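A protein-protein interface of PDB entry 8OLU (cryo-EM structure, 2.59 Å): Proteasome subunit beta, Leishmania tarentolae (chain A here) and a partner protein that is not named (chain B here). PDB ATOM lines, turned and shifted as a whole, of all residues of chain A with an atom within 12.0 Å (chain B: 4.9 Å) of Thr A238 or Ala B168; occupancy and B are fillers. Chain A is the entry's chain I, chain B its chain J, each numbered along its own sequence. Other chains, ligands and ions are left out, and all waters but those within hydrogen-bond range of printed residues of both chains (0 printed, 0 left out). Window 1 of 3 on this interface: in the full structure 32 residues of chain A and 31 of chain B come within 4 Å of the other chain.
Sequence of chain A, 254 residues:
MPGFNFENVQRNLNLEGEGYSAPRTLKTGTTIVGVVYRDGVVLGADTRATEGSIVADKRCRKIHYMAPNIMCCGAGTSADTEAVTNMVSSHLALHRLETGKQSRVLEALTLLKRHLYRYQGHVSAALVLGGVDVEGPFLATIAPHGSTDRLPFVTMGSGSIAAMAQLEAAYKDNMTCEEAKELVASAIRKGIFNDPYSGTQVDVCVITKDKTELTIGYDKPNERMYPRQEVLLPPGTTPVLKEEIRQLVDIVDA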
ATOM      1  N   VAL A 231      30.881 -34.598 -13.916  1.00  0.00           N
ATOM      2  CA  VAL A 231      29.907 -33.832 -14.674  1.00  0.00           C
ATOM      3  C   VAL A 231      29.986 -32.378 -14.209  1.00  0.00           C
ATOM      4  O   VAL A 231      29.778 -32.094 -13.036  1.00  0.00           O
ATOM      5  CB  VAL A 231      28.481 -34.393 -14.473  1.00  0.00           C
ATOM      6  CG1 VAL A 231      27.437 -33.535 -15.186  1.00  0.00           C
ATOM      7  CG2 VAL A 231      28.361 -35.868 -14.870  1.00  0.00           C
ATOM      8  N   LEU A 232      30.278 -31.461 -15.134  1.00  0.00           N
ATOM      9  CA  LEU A 232      30.534 -30.077 -14.775  1.00  0.00           C
ATOM     10  C   LEU A 232      29.216 -29.301 -14.752  1.00  0.00           C
ATOM     11  O   LEU A 232      28.556 -29.129 -15.786  1.00  0.00           O
ATOM     12  CB  LEU A 232      31.537 -29.478 -15.772  1.00  0.00           C
ATOM     13  CG  LEU A 232      32.101 -28.100 -15.412  1.00  0.00           C
ATOM     14  CD1 LEU A 232      32.936 -28.161 -14.131  1.00  0.00           C
ATOM     15  CD2 LEU A 232      32.911 -27.526 -16.574  1.00  0.00           C
ATOM     16  N   LEU A 233      28.858 -28.835 -13.544  1.00  0.00           N
ATOM     17  CA  LEU A 233      27.681 -28.006 -13.324  1.00  0.00           C
ATOM     18  C   LEU A 233      28.121 -26.715 -12.621  1.00  0.00           C
ATOM     19  O   LEU A 233      28.205 -26.642 -11.395  1.00  0.00           O
ATOM     20  CB  LEU A 233      26.646 -28.821 -12.529  1.00  0.00           C
ATOM     21  CG  LEU A 233      26.092 -30.077 -13.228  1.00  0.00           C
ATOM     22  CD1 LEU A 233      25.057 -30.788 -12.372  1.00  0.00           C
ATOM     23  CD2 LEU A 233      25.489 -29.758 -14.587  1.00  0.00           C
ATOM     24  N   PRO A 234      28.474 -25.664 -13.402  1.00  0.00           N
ATOM     25  CA  PRO A 234      29.034 -24.431 -12.839  1.00  0.00           C
ATOM     26  C   PRO A 234      28.002 -23.545 -12.165  1.00  0.00           C
ATOM     27  O   PRO A 234      26.914 -23.368 -12.699  1.00  0.00           O
ATOM     28  CB  PRO A 234      29.546 -23.660 -14.064  1.00  0.00           C
ATOM     29  CG  PRO A 234      28.717 -24.202 -15.230  1.00  0.00           C
ATOM     30  CD  PRO A 234      28.382 -25.637 -14.876  1.00  0.00           C
ATOM     31  N   PRO A 235      28.301 -22.931 -11.004  1.00  0.00           N
ATOM     32  CA  PRO A 235      27.344 -22.027 -10.356  1.00  0.00           C
ATOM     33  C   PRO A 235      26.462 -21.210 -11.312  1.00  0.00           C
ATOM     34  O   PRO A 235      26.917 -20.766 -12.368  1.00  0.00           O
ATOM     35  CB  PRO A 235      28.287 -21.148  -9.522  1.00  0.00           C
ATOM     36  CG  PRO A 235      29.380 -22.126  -9.089  1.00  0.00           C
ATOM     37  CD  PRO A 235      29.550 -23.098 -10.241  1.00  0.00           C
ATOM     38  N   GLY A 236      25.187 -21.041 -10.918  1.00  0.00           N
ATOM     39  CA  GLY A 236      24.175 -20.345 -11.695  1.00  0.00           C
ATOM     40  C   GLY A 236      23.505 -21.251 -12.732  1.00  0.00           C
ATOM     41  O   GLY A 236      22.561 -20.831 -13.406  1.00  0.00           O
ATOM     42  N   THR A 237      24.002 -22.491 -12.857  1.00  0.00           N
ATOM     43  CA  THR A 237      23.490 -23.463 -13.819  1.00  0.00           C
ATOM     44  C   THR A 237      22.020 -23.776 -13.568  1.00  0.00           C
ATOM     45  O   THR A 237      21.278 -24.048 -14.511  1.00  0.00           O
ATOM     46  CB  THR A 237      24.355 -24.738 -13.838  1.00  0.00           C
ATOM     47  OG1 THR A 237      25.199 -24.680 -14.997  1.00  0.00           O
ATOM     48  CG2 THR A 237      23.591 -26.033 -13.929  1.00  0.00           C
ATOM     49  N   THR A 238      21.607 -23.793 -12.299  1.00  0.00           N
ATOM     50  CA  THR A 238      20.249 -24.188 -11.979  1.00  0.00           C
ATOM     51  C   THR A 238      19.437 -22.921 -11.721  1.00  0.00           C
ATOM     52  O   THR A 238      19.856 -22.072 -10.943  1.00  0.00           O
ATOM     53  CB  THR A 238      20.204 -25.208 -10.828  1.00  0.00           C
ATOM     54  OG1 THR A 238      21.056 -26.331 -11.082  1.00  0.00           O
ATOM     55  CG2 THR A 238      18.803 -25.741 -10.615  1.00  0.00           C
ATOM     56  N   PRO A 239      18.252 -22.770 -12.363  1.00  0.00           N
ATOM     57  CA  PRO A 239      17.419 -21.573 -12.226  1.00  0.00           C
ATOM     58  C   PRO A 239      16.782 -21.432 -10.857  1.00  0.00           C
ATOM     59  O   PRO A 239      16.037 -22.297 -10.400  1.00  0.00           O
ATOM     60  CB  PRO A 239      16.288 -21.734 -13.246  1.00  0.00           C
ATOM     61  CG  PRO A 239      16.748 -22.872 -14.160  1.00  0.00           C
ATOM     62  CD  PRO A 239      17.642 -23.735 -13.286  1.00  0.00           C
ATOM     63  N   VAL A 240      17.115 -20.308 -10.233  1.00  0.00           N
ATOM     64  CA  VAL A 240      16.651 -19.962  -8.914  1.00  0.00           C
ATOM     65  C   VAL A 240      15.663 -18.821  -9.061  1.00  0.00           C
ATOM     66  O   VAL A 240      15.810 -17.991  -9.957  1.00  0.00           O
ATOM     67  CB  VAL A 240      17.847 -19.626  -8.009  1.00  0.00           C
ATOM     68  CG1 VAL A 240      17.423 -19.030  -6.673  1.00  0.00           C
ATOM     69  CG2 VAL A 240      18.705 -20.865  -7.778  1.00  0.00           C
ATOM     70  N   LEU A 241      14.638 -18.857  -8.207  1.00  0.00           N
ATOM     71  CA  LEU A 241      13.527 -17.929  -8.221  1.00  0.00           C
ATOM     72  C   LEU A 241      13.715 -16.884  -7.133  1.00  0.00           C
ATOM     73  O   LEU A 241      13.469 -15.703  -7.351  1.00  0.00           O
ATOM     74  CB  LEU A 241      12.226 -18.689  -7.962  1.00  0.00           C
ATOM     75  CG  LEU A 241      11.707 -19.599  -9.076  1.00  0.00           C
ATOM     76  CD1 LEU A 241      10.248 -20.004  -8.782  1.00  0.00           C
ATOM     77  CD2 LEU A 241      11.843 -18.942 -10.463  1.00  0.00           C
ATOM     78  N   LYS A 242      14.043 -17.367  -5.937  1.00  0.00           N
ATOM     79  CA  LYS A 242      14.277 -16.523  -4.783  1.00  0.00           C
ATOM     80  C   LYS A 242      15.435 -17.120  -4.005  1.00  0.00           C
ATOM     81  O   LYS A 242      15.798 -18.272  -4.215  1.00  0.00           O
ATOM     82  CB  LYS A 242      13.055 -16.444  -3.871  1.00  0.00           C
ATOM     83  CG  LYS A 242      11.781 -15.944  -4.530  1.00  0.00           C
ATOM     84  CD  LYS A 242      10.597 -15.861  -3.555  1.00  0.00           C
ATOM     85  CE  LYS A 242       9.692 -14.677  -3.838  1.00  0.00           C
ATOM     86  NZ  LYS A 242       8.374 -14.820  -3.178  1.00  0.00           N
ATOM     87  N   GLU A 243      15.966 -16.308  -3.090  1.00  0.00           N
ATOM     88  CA  GLU A 243      17.168 -16.606  -2.338  1.00  0.00           C
ATOM     89  C   GLU A 243      17.068 -15.822  -1.050  1.00  0.00           C
ATOM     90  O   GLU A 243      16.653 -14.676  -1.072  1.00  0.00           O
ATOM     91  CB  GLU A 243      18.396 -16.204  -3.156  1.00  0.00           C
ATOM     92  CG  GLU A 243      19.718 -16.613  -2.522  1.00  0.00           C
ATOM     93  CD  GLU A 243      20.856 -16.946  -3.485  1.00  0.00           C
ATOM     94  OE1 GLU A 243      20.588 -17.603  -4.527  1.00  0.00           O
ATOM     95  OE2 GLU A 243      22.024 -16.614  -3.160  1.00  0.00           O
ATOM     96  N   ILE B  23      17.413 -30.467   0.544  1.00  0.00           N
ATOM     97  CA  ILE B  23      16.493 -29.994  -0.420  1.00  0.00           C
ATOM     98  C   ILE B  23      15.206 -30.784  -0.435  1.00  0.00           C
ATOM     99  O   ILE B  23      15.216 -31.992  -0.340  1.00  0.00           O
ATOM    100  CB  ILE B  23      17.185 -30.027  -1.768  1.00  0.00           C
ATOM    101  CG1 ILE B  23      16.232 -29.539  -2.847  1.00  0.00           C
ATOM    102  CG2 ILE B  23      17.635 -31.442  -2.131  1.00  0.00           C
ATOM    103  CD1 ILE B  23      16.990 -29.264  -4.134  1.00  0.00           C
ATOM    104  N   PHE B 164      25.192 -27.335  -4.145  1.00  0.00           N
ATOM    105  CA  PHE B 164      23.885 -26.859  -4.534  1.00  0.00           C
ATOM    106  C   PHE B 164      23.550 -27.255  -5.975  1.00  0.00           C
ATOM    107  O   PHE B 164      22.546 -27.926  -6.213  1.00  0.00           O
ATOM    108  CB  PHE B 164      23.798 -25.360  -4.314  1.00  0.00           C
ATOM    109  CG  PHE B 164      22.499 -24.838  -4.826  1.00  0.00           C
ATOM    110  CD1 PHE B 164      21.335 -25.049  -4.105  1.00  0.00           C
ATOM    111  CD2 PHE B 164      22.421 -24.310  -6.098  1.00  0.00           C
ATOM    112  CE1 PHE B 164      20.109 -24.665  -4.619  1.00  0.00           C
ATOM    113  CE2 PHE B 164      21.194 -23.899  -6.594  1.00  0.00           C
ATOM    114  CZ  PHE B 164      20.044 -24.082  -5.852  1.00  0.00           C
ATOM    115  N   GLU B 165      24.390 -26.959  -6.950  1.00  0.00           N
ATOM    116  CA  GLU B 165      24.000 -27.313  -8.304  1.00  0.00           C
ATOM    117  C   GLU B 165      23.713 -28.794  -8.457  1.00  0.00           C
ATOM    118  O   GLU B 165      22.804 -29.172  -9.180  1.00  0.00           O
ATOM    119  CB  GLU B 165      25.006 -26.867  -9.359  1.00  0.00           C
ATOM    120  CG  GLU B 165      25.220 -25.350  -9.328  1.00  0.00           C
ATOM    121  CD  GLU B 165      23.974 -24.470  -9.533  1.00  0.00           C
ATOM    122  OE1 GLU B 165      23.950 -23.273  -9.041  1.00  0.00           O
ATOM    123  OE2 GLU B 165      23.017 -24.958 -10.213  1.00  0.00           O
ATOM    124  N   ILE B 166      24.469 -29.660  -7.822  1.00  0.00           N
ATOM    125  CA  ILE B 166      24.206 -31.046  -8.119  1.00  0.00           C
ATOM    126  C   ILE B 166      23.038 -31.511  -7.261  1.00  0.00           C
ATOM    127  O   ILE B 166      22.275 -32.406  -7.661  1.00  0.00           O
ATOM    128  CB  ILE B 166      25.461 -31.935  -8.025  1.00  0.00           C
ATOM    129  CG1 ILE B 166      25.752 -32.380  -6.602  1.00  0.00           C
ATOM    130  CG2 ILE B 166      26.669 -31.272  -8.660  1.00  0.00           C
ATOM    131  CD1 ILE B 166      25.134 -33.728  -6.288  1.00  0.00           C
ATOM    132  N   ALA B 167      22.839 -30.889  -6.104  1.00  0.00           N
ATOM    133  CA  ALA B 167      21.636 -31.203  -5.364  1.00  0.00           C
ATOM    134  C   ALA B 167      20.421 -30.812  -6.203  1.00  0.00           C
ATOM    135  O   ALA B 167      19.545 -31.630  -6.417  1.00  0.00           O
ATOM    136  CB  ALA B 167      21.618 -30.543  -4.013  1.00  0.00           C
ATOM    137  N   ALA B 168      20.371 -29.592  -6.711  1.00  0.00           N
ATOM    138  CA  ALA B 168      19.196 -29.192  -7.463  1.00  0.00           C
ATOM    139  C   ALA B 168      18.965 -30.027  -8.718  1.00  0.00           C
ATOM    140  O   ALA B 168      17.863 -30.528  -8.912  1.00  0.00           O
ATOM    141  CB  ALA B 168      19.318 -27.783  -7.825  1.00  0.00           C
ATOM    142  N   GLN B 169      19.987 -30.230  -9.544  1.00  0.00           N
ATOM    143  CA  GLN B 169      19.800 -31.050 -10.722  1.00  0.00           C
ATOM    144  C   GLN B 169      19.284 -32.431 -10.369  1.00  0.00           C
ATOM    145  O   GLN B 169      18.511 -33.039 -11.107  1.00  0.00           O
ATOM    146  CB  GLN B 169      21.071 -31.173 -11.560  1.00  0.00           C
ATOM    147  CG  GLN B 169      21.473 -29.834 -12.179  1.00  0.00           C
ATOM    148  CD  GLN B 169      20.400 -29.253 -13.071  1.00  0.00           C
ATOM    149  OE1 GLN B 169      19.775 -29.975 -13.866  1.00  0.00           O
ATOM    150  NE2 GLN B 169      20.178 -27.949 -12.920  1.00  0.00           N
ATOM    151  N   ALA B 170      19.742 -32.929  -9.249  1.00  0.00           N
ATOM    152  CA  ALA B 170      19.350 -34.271  -8.847  1.00  0.00           C
ATOM    153  C   ALA B 170      17.903 -34.272  -8.371  1.00  0.00           C
ATOM    154  O   ALA B 170      17.107 -35.109  -8.817  1.00  0.00           O
ATOM    155  CB  ALA B 170      20.307 -34.775  -7.785  1.00  0.00           C
ATOM    156  N   MET B 171      17.560 -33.308  -7.523  1.00  0.00           N
ATOM    157  CA  MET B 171      16.197 -33.268  -7.039  1.00  0.00           C
ATOM    158  C   MET B 171      15.251 -33.095  -8.220  1.00  0.00           C
ATOM    159  O   MET B 171      14.297 -33.855  -8.332  1.00  0.00           O
ATOM    160  CB  MET B 171      15.958 -32.180  -5.987  1.00  0.00           C
ATOM    161  CG  MET B 171      14.483 -32.042  -5.571  1.00  0.00           C
ATOM    162  SD  MET B 171      13.682 -33.540  -4.840  1.00  0.00           S
ATOM    163  CE  MET B 171      14.629 -33.778  -3.337  1.00  0.00           C
ATOM    164  N   LEU B 172      15.531 -32.151  -9.114  1.00  0.00           N
ATOM    165  CA  LEU B 172      14.667 -31.940 -10.269  1.00  0.00           C
ATOM    166  C   LEU B 172      14.647 -33.088 -11.239  1.00  0.00           C
ATOM    167  O   LEU B 172      13.622 -33.482 -11.720  1.00  0.00           O
ATOM    168  CB  LEU B 172      15.166 -30.734 -11.028  1.00  0.00           C
ATOM    169  CG  LEU B 172      15.175 -29.447 -10.221  1.00  0.00           C
ATOM    170  CD1 LEU B 172      15.765 -28.312 -11.017  1.00  0.00           C
ATOM    171  CD2 LEU B 172      13.775 -29.133  -9.826  1.00  0.00           C
ATOM    172  N   SER B 173      15.777 -33.639 -11.577  1.00  0.00           N
ATOM    173  CA  SER B 173      15.730 -34.726 -12.535  1.00  0.00           C
ATOM    174  C   SER B 173      14.921 -35.877 -11.985  1.00  0.00           C
ATOM    175  O   SER B 173      14.237 -36.569 -12.707  1.00  0.00           O
ATOM    176  CB  SER B 173      17.103 -35.134 -12.941  1.00  0.00           C
ATOM    177  OG  SER B 173      17.801 -33.996 -13.452  1.00  0.00           O
ATOM    178  N   ILE B 200      13.850 -23.060  -6.035  1.00  0.00           N
ATOM    179  CA  ILE B 200      14.331 -23.478  -7.315  1.00  0.00           C
ATOM    180  C   ILE B 200      13.124 -23.726  -8.183  1.00  0.00           C
ATOM    181  O   ILE B 200      12.155 -24.335  -7.740  1.00  0.00           O
ATOM    182  CB  ILE B 200      15.090 -24.791  -7.097  1.00  0.00           C
ATOM    183  CG1 ILE B 200      16.328 -24.560  -6.264  1.00  0.00           C
ATOM    184  CG2 ILE B 200      15.451 -25.549  -8.377  1.00  0.00           C
ATOM    185  CD1 ILE B 200      16.836 -25.880  -5.735  1.00  0.00           C
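The side-chain hydroxyl (OG) of Ser B173 lies within hydrogen-bond range of the backbone carbonyl oxygen (O) of Gln B169 (2.6 Å).
O of Pro A234 sits close to OG1 of Thr A237 (3.2 Å).
Of the 12 printed residues of chain B, 5 touch a printed residue of chain A.
Hydrophobic or aromatic side chains of chain B that line the printed part of chain A: Phe B164, Ala B168 and Ile B200.
Among the printed residues, 10 pairs touch across the chains.
Among the printed residues, no Asp or Glu carboxylate lies within 4 Å of a Lys or Arg side-chain nitrogen of the other chain.
Among the printed residues, pairs that only touch across the chains: Leu A233 with Glu B165 (3.8 Å), Leu A233 with Gln B169 (3.7 Å), Pro A235 with Glu B165 (3.8 Å), Thr A237 with Glu B165 (3.7 Å), Thr A238 with Ala B168 (3.5 Å), Pro A239 with Ile B200 (3.7 Å) and Val A240 with Phe B164 (3.98 Å).
Of the printed residues of chain B, Thr A238 touches Glu B165 (2.5 Å), Ala B168 (3.5 Å) and Gln B169 (2.6 Å).
Ala B168 touches just one residue of chain A: Thr A238.
Glu B165 touches just these residues of chain A: Leu A233 (3.8 Å), Pro A235 (3.8 Å), Gly A236 (3.2 Å), Thr A237 (3.7 Å) and Thr A238 (2.5 Å).
No residue of chain A comes within 4 Å of Ile B166.
No residue of chain A comes within 4 Å of Ala B167.
Of chain A, only Leu A233 (3.7 Å) and Thr A238 (2.6 Å) come within 4 Å of Gln B169.
Ala B170 touches none of the printed residues of chain A.
No residue of chain A comes within 4 Å of Met B171.
Of chain A, only Pro A239 (3.7 Å) comes within 4 Å of Ile B200.
Printed residues of chain A within 4 Å of Phe B164: Val A240 (3.98 Å).
Printed residues of chain B within 4 Å of Pro A239: Ile B200.
Of the printed residues of chain B, Leu A233 touches Glu B165 (3.8 Å) and Gln B169 (3.7 Å).
Printed residues of chain B within 4 Å of Gly A236: Glu B165 (3.2 Å).
The nearest residue of chain A that does not touch Ala B168 is Pro A239 (6.8 Å).
The nearest printed residue of chain B that does not touch Gly A236 is Phe B164 (6.4 Å).
The backbone NH (N) of Gly A236 is in hydrogen-bond range of the side-chain carboxylate (OE1) of Glu B165, at 3.2 Å.
OE2 of Glu B165 is in hydrogen-bond range of OG1 of Thr A238 (2.5 Å).
The side-chain amide nitrogen (NE2) of Gln B169 lies within hydrogen-bond range of the side-chain hydroxyl (OG1) of Thr A238, at 2.6 Å.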
